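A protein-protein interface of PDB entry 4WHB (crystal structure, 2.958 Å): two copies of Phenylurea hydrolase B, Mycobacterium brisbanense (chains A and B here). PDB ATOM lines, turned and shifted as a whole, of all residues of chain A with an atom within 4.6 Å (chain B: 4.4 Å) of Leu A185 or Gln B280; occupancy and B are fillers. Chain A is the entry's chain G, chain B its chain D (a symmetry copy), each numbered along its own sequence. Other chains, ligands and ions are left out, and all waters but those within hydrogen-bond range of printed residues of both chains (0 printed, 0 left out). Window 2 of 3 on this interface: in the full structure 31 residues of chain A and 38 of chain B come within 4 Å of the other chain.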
ATOM      1  N   GLN A 181      18.844  -5.356  -9.520  1.00  0.00           N
ATOM      2  CA  GLN A 181      20.023  -6.016 -10.024  1.00  0.00           C
ATOM      3  C   GLN A 181      19.496  -7.358 -10.334  1.00  0.00           C
ATOM      4  O   GLN A 181      18.338  -7.582 -10.074  1.00  0.00           O
ATOM      5  CB  GLN A 181      21.123  -6.084  -8.989  1.00  0.00           C
ATOM      6  CG  GLN A 181      22.319  -6.930  -9.429  1.00  0.00           C
ATOM      7  CD  GLN A 181      23.635  -6.625  -8.741  1.00  0.00           C
ATOM      8  OE1 GLN A 181      24.522  -6.042  -9.323  1.00  0.00           O
ATOM      9  NE2 GLN A 181      23.775  -7.054  -7.521  1.00  0.00           N
ATOM     10  N   LEU A 182      20.298  -8.191 -10.971  1.00  0.00           N
ATOM     11  CA  LEU A 182      19.952  -9.511 -11.421  1.00  0.00           C
ATOM     12  C   LEU A 182      19.651  -9.311 -12.836  1.00  0.00           C
ATOM     13  O   LEU A 182      19.587 -10.215 -13.579  1.00  0.00           O
ATOM     14  CB  LEU A 182      18.750 -10.166 -10.720  1.00  0.00           C
ATOM     15  CG  LEU A 182      18.394 -10.134  -9.211  1.00  0.00           C
ATOM     16  CD1 LEU A 182      16.984  -9.646  -8.984  1.00  0.00           C
ATOM     17  CD2 LEU A 182      18.562 -11.463  -8.524  1.00  0.00           C
ATOM     18  N   SER A 183      19.488  -8.083 -13.230  1.00  0.00           N
ATOM     19  CA  SER A 183      19.532  -7.820 -14.641  1.00  0.00           C
ATOM     20  C   SER A 183      20.953  -8.194 -15.070  1.00  0.00           C
ATOM     21  O   SER A 183      21.174  -8.770 -16.138  1.00  0.00           O
ATOM     22  CB  SER A 183      19.273  -6.333 -14.890  1.00  0.00           C
ATOM     23  OG  SER A 183      20.475  -5.577 -14.948  1.00  0.00           O
ATOM     24  N   LEU A 184      21.906  -7.809 -14.209  1.00  0.00           N
ATOM     25  CA  LEU A 184      23.330  -8.120 -14.297  1.00  0.00           C
ATOM     26  C   LEU A 184      23.865  -9.537 -13.985  1.00  0.00           C
ATOM     27  O   LEU A 184      24.726 -10.053 -14.708  1.00  0.00           O
ATOM     28  CB  LEU A 184      24.041  -7.123 -13.403  1.00  0.00           C
ATOM     29  CG  LEU A 184      23.806  -5.645 -13.756  1.00  0.00           C
ATOM     30  CD1 LEU A 184      24.347  -4.877 -12.564  1.00  0.00           C
ATOM     31  CD2 LEU A 184      24.554  -5.180 -15.002  1.00  0.00           C
ATOM     32  N   LEU A 185      23.400 -10.154 -12.916  1.00  0.00           N
ATOM     33  CA  LEU A 185      23.904 -11.443 -12.470  1.00  0.00           C
ATOM     34  C   LEU A 185      23.775 -12.526 -13.535  1.00  0.00           C
ATOM     35  O   LEU A 185      22.774 -12.564 -14.252  1.00  0.00           O
ATOM     36  CB  LEU A 185      23.159 -11.894 -11.209  1.00  0.00           C
ATOM     37  CG  LEU A 185      23.582 -11.478  -9.810  1.00  0.00           C
ATOM     38  CD1 LEU A 185      22.492 -11.772  -8.810  1.00  0.00           C
ATOM     39  CD2 LEU A 185      24.788 -12.324  -9.450  1.00  0.00           C
ATOM     40  N   PRO A 186      24.800 -13.399 -13.643  1.00  0.00           N
ATOM     41  CA  PRO A 186      24.640 -14.627 -14.399  1.00  0.00           C
ATOM     42  C   PRO A 186      23.523 -15.425 -13.755  1.00  0.00           C
ATOM     43  O   PRO A 186      23.395 -15.443 -12.517  1.00  0.00           O
ATOM     44  CB  PRO A 186      25.984 -15.326 -14.220  1.00  0.00           C
ATOM     45  CG  PRO A 186      26.654 -14.663 -13.036  1.00  0.00           C
ATOM     46  CD  PRO A 186      26.136 -13.277 -13.005  1.00  0.00           C
ATOM     47  N   ARG A 187      22.704 -16.066 -14.565  1.00  0.00           N
ATOM     48  CA  ARG A 187      21.429 -16.580 -14.070  1.00  0.00           C
ATOM     49  C   ARG A 187      21.517 -17.707 -13.061  1.00  0.00           C
ATOM     50  O   ARG A 187      20.599 -17.891 -12.256  1.00  0.00           O
ATOM     51  CB  ARG A 187      20.561 -17.050 -15.235  1.00  0.00           C
ATOM     52  CG  ARG A 187      20.897 -18.448 -15.746  1.00  0.00           C
ATOM     53  CD  ARG A 187      20.082 -18.765 -16.977  1.00  0.00           C
ATOM     54  NE  ARG A 187      20.688 -18.221 -18.179  1.00  0.00           N
ATOM     55  CZ  ARG A 187      21.421 -18.896 -19.006  1.00  0.00           C
ATOM     56  NH1 ARG A 187      21.648 -20.180 -18.781  1.00  0.00           N
ATOM     57  NH2 ARG A 187      21.888 -18.259 -20.073  1.00  0.00           N
ATOM     58  N   GLU A 189      23.623 -17.944 -10.656  1.00  0.00           N
ATOM     59  CA  GLU A 189      23.708 -17.288  -9.362  1.00  0.00           C
ATOM     60  C   GLU A 189      22.436 -16.500  -9.061  1.00  0.00           C
ATOM     61  O   GLU A 189      22.148 -16.216  -7.885  1.00  0.00           O
ATOM     62  CB  GLU A 189      24.959 -16.403  -9.281  1.00  0.00           C
ATOM     63  CG  GLU A 189      26.286 -17.184  -9.374  1.00  0.00           C
ATOM     64  CD  GLU A 189      26.676 -17.900  -8.075  1.00  0.00           C
ATOM     65  OE1 GLU A 189      25.829 -17.934  -7.145  1.00  0.00           O
ATOM     66  OE2 GLU A 189      27.830 -18.431  -7.984  1.00  0.00           O
ATOM     67  N   VAL A 190      21.678 -16.138 -10.092  1.00  0.00           N
ATOM     68  CA  VAL A 190      20.323 -15.592  -9.866  1.00  0.00           C
ATOM     69  C   VAL A 190      19.461 -16.693  -9.268  1.00  0.00           C
ATOM     70  O   VAL A 190      18.612 -16.442  -8.426  1.00  0.00           O
ATOM     71  CB  VAL A 190      19.645 -15.068 -11.145  1.00  0.00           C
ATOM     72  CG1 VAL A 190      18.210 -14.616 -10.834  1.00  0.00           C
ATOM     73  CG2 VAL A 190      20.452 -13.922 -11.755  1.00  0.00           C
ATOM     74  N   ARG A 193      19.328 -16.497  -5.636  1.00  0.00           N
ATOM     75  CA  ARG A 193      18.649 -15.382  -4.984  1.00  0.00           C
ATOM     76  C   ARG A 193      17.204 -15.211  -5.341  1.00  0.00           C
ATOM     77  O   ARG A 193      16.564 -14.329  -4.748  1.00  0.00           O
ATOM     78  CB  ARG A 193      19.402 -14.098  -5.223  1.00  0.00           C
ATOM     79  CG  ARG A 193      20.859 -14.194  -4.730  1.00  0.00           C
ATOM     80  CD  ARG A 193      21.375 -12.902  -4.079  1.00  0.00           C
ATOM     81  NE  ARG A 193      22.464 -12.306  -4.856  1.00  0.00           N
ATOM     82  CZ  ARG A 193      22.635 -11.000  -5.032  1.00  0.00           C
ATOM     83  NH1 ARG A 193      21.804 -10.123  -4.508  1.00  0.00           N
ATOM     84  NH2 ARG A 193      23.656 -10.550  -5.741  1.00  0.00           N
ATOM     85  N   VAL B 257      25.730  -9.799 -18.445  1.00  0.00           N
ATOM     86  CA  VAL B 257      26.333 -11.133 -18.553  1.00  0.00           C
ATOM     87  C   VAL B 257      25.438 -12.065 -19.353  1.00  0.00           C
ATOM     88  O   VAL B 257      25.938 -13.008 -20.024  1.00  0.00           O
ATOM     89  CB  VAL B 257      26.572 -11.768 -17.170  1.00  0.00           C
ATOM     90  CG1 VAL B 257      27.366 -13.070 -17.303  1.00  0.00           C
ATOM     91  CG2 VAL B 257      27.290 -10.777 -16.239  1.00  0.00           C
ATOM     92  N   GLU B 258      24.132 -11.803 -19.310  1.00  0.00           N
ATOM     93  CA  GLU B 258      23.210 -12.350 -20.330  1.00  0.00           C
ATOM     94  C   GLU B 258      23.478 -11.446 -21.534  1.00  0.00           C
ATOM     95  O   GLU B 258      24.619 -11.018 -21.683  1.00  0.00           O
ATOM     96  CB  GLU B 258      21.759 -12.314 -19.874  1.00  0.00           C
ATOM     97  CG  GLU B 258      21.485 -12.931 -18.508  1.00  0.00           C
ATOM     98  CD  GLU B 258      21.689 -14.413 -18.481  1.00  0.00           C
ATOM     99  OE1 GLU B 258      20.961 -15.103 -19.252  1.00  0.00           O
ATOM    100  OE2 GLU B 258      22.560 -14.860 -17.678  1.00  0.00           O
ATOM    101  N   THR B 277      30.456  -6.297 -19.124  1.00  0.00           N
ATOM    102  CA  THR B 277      29.275  -6.978 -18.609  1.00  0.00           C
ATOM    103  C   THR B 277      28.748  -6.217 -17.395  1.00  0.00           C
ATOM    104  O   THR B 277      27.772  -6.638 -16.759  1.00  0.00           O
ATOM    105  CB  THR B 277      29.648  -8.418 -18.204  1.00  0.00           C
ATOM    106  OG1 THR B 277      30.913  -8.434 -17.492  1.00  0.00           O
ATOM    107  CG2 THR B 277      29.769  -9.283 -19.469  1.00  0.00           C
ATOM    108  N   LEU B 278      29.400  -5.095 -17.065  1.00  0.00           N
ATOM    109  CA  LEU B 278      28.988  -4.202 -15.986  1.00  0.00           C
ATOM    110  C   LEU B 278      28.957  -4.817 -14.591  1.00  0.00           C
ATOM    111  O   LEU B 278      27.901  -5.097 -14.058  1.00  0.00           O
ATOM    112  CB  LEU B 278      27.650  -3.548 -16.300  1.00  0.00           C
ATOM    113  CG  LEU B 278      27.654  -2.562 -17.469  1.00  0.00           C
ATOM    114  CD1 LEU B 278      26.540  -1.517 -17.306  1.00  0.00           C
ATOM    115  CD2 LEU B 278      28.984  -1.866 -17.640  1.00  0.00           C
ATOM    116  N   GLY B 279      30.125  -5.050 -14.014  1.00  0.00           N
ATOM    117  CA  GLY B 279      30.273  -5.247 -12.575  1.00  0.00           C
ATOM    118  C   GLY B 279      30.425  -6.727 -12.292  1.00  0.00           C
ATOM    119  O   GLY B 279      30.664  -7.117 -11.154  1.00  0.00           O
ATOM    120  N   GLN B 280      30.265  -7.535 -13.334  1.00  0.00           N
ATOM    121  CA  GLN B 280      30.451  -8.961 -13.240  1.00  0.00           C
ATOM    122  C   GLN B 280      31.568  -9.369 -14.175  1.00  0.00           C
ATOM    123  O   GLN B 280      31.919  -8.672 -15.105  1.00  0.00           O
ATOM    124  CB  GLN B 280      29.164  -9.683 -13.645  1.00  0.00           C
ATOM    125  CG  GLN B 280      28.418 -10.364 -12.506  1.00  0.00           C
ATOM    126  CD  GLN B 280      27.830  -9.404 -11.484  1.00  0.00           C
ATOM    127  OE1 GLN B 280      27.763  -8.176 -11.693  1.00  0.00           O
ATOM    128  NE2 GLN B 280      27.356  -9.979 -10.369  1.00  0.00           N
ATOM    129  N   GLU B 281      32.119 -10.545 -13.920  1.00  0.00           N
ATOM    130  CA  GLU B 281      33.167 -11.125 -14.749  1.00  0.00           C
ATOM    131  C   GLU B 281      32.518 -12.256 -15.531  1.00  0.00           C
ATOM    132  O   GLU B 281      31.781 -13.062 -14.984  1.00  0.00           O
ATOM    133  CB  GLU B 281      34.331 -11.627 -13.875  1.00  0.00           C
ATOM    134  CG  GLU B 281      34.807 -10.553 -12.915  1.00  0.00           C
ATOM    135  CD  GLU B 281      35.738 -11.048 -11.830  1.00  0.00           C
ATOM    136  OE1 GLU B 281      36.865 -11.376 -12.212  1.00  0.00           O
ATOM    137  OE2 GLU B 281      35.376 -11.089 -10.609  1.00  0.00           O
ATOM    138  N   ILE B 282      32.794 -12.303 -16.823  1.00  0.00           N
ATOM    139  CA  ILE B 282      32.166 -13.299 -17.680  1.00  0.00           C
ATOM    140  C   ILE B 282      32.574 -14.695 -17.172  1.00  0.00           C
ATOM    141  O   ILE B 282      33.811 -14.965 -17.016  1.00  0.00           O
ATOM    142  CB  ILE B 282      32.598 -13.194 -19.158  1.00  0.00           C
ATOM    143  CG1 ILE B 282      33.214 -11.850 -19.481  1.00  0.00           C
ATOM    144  CG2 ILE B 282      31.405 -13.505 -20.052  1.00  0.00           C
ATOM    145  CD1 ILE B 282      33.403 -11.589 -20.959  1.00  0.00           C
ATOM    146  N   PRO B 324      35.739  -4.763 -12.668  1.00  0.00           N
ATOM    147  CA  PRO B 324      35.656  -6.068 -13.300  1.00  0.00           C
ATOM    148  C   PRO B 324      35.876  -5.954 -14.796  1.00  0.00           C
ATOM    149  O   PRO B 324      36.241  -6.942 -15.435  1.00  0.00           O
ATOM    150  CB  PRO B 324      34.243  -6.503 -13.011  1.00  0.00           C
ATOM    151  CG  PRO B 324      33.950  -5.857 -11.709  1.00  0.00           C
ATOM    152  CD  PRO B 324      34.601  -4.507 -11.793  1.00  0.00           C
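The guanidinium group (NE) of Arg A187 is in salt-bridge range of the side-chain carboxylate (OE1) of Glu B258, at 3.3 Å.
Printed residues of chain B that touch a printed residue of chain A: Val B257, Glu B258, Thr B277, Leu B278 and Gln B280. Among the printed residues, Asp or Glu carboxylates within 4 Å of a Lys or Arg side-chain nitrogen of the other chain: Arg A187 with Glu B258 (3.3 Å).
Leu A185 touches just one residue of chain B: Gln B280. Of chain A, only Leu A185 and Pro A186 come within 4 Å of Gln B280. Of the printed residues of chain B, Leu A184 touches Val B257, Thr B277 and Leu B278. Printed residues of chain A within 4 Å of Val B257: Leu A184. Of the printed residues of chain A, Leu B278 touches Leu A184. Printed residues of chain B within 4 Å of Pro A186: Glu B258 (3.9 Å) and Gln B280 (3.7 Å). Of the printed residues of chain B, Arg A187 touches Glu B258 (3.3 Å). The nearest residue of chain B that does not touch Leu A185 is Glu B258 (4.1 Å). The nearest printed residue of chain B that does not touch Pro A186 is Val B257 (4.1 Å).
The side-chain hydroxyl (OG1) of Thr B277 sits at hydrogen-bond distance from the backbone carbonyl oxygen (O) of Gln B280 (2.6 Å).
No position is printed for both chains.
Leu A184 touches Val B257. Leu A184 touches Thr B277. Leu B278 touches Leu A184 (O to CD2, 3.5 Å). Gln B280 touches Leu A185. Glu B258 touches Pro A186. CD of Pro A186 touches CG of Gln B280 (3.7 Å).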
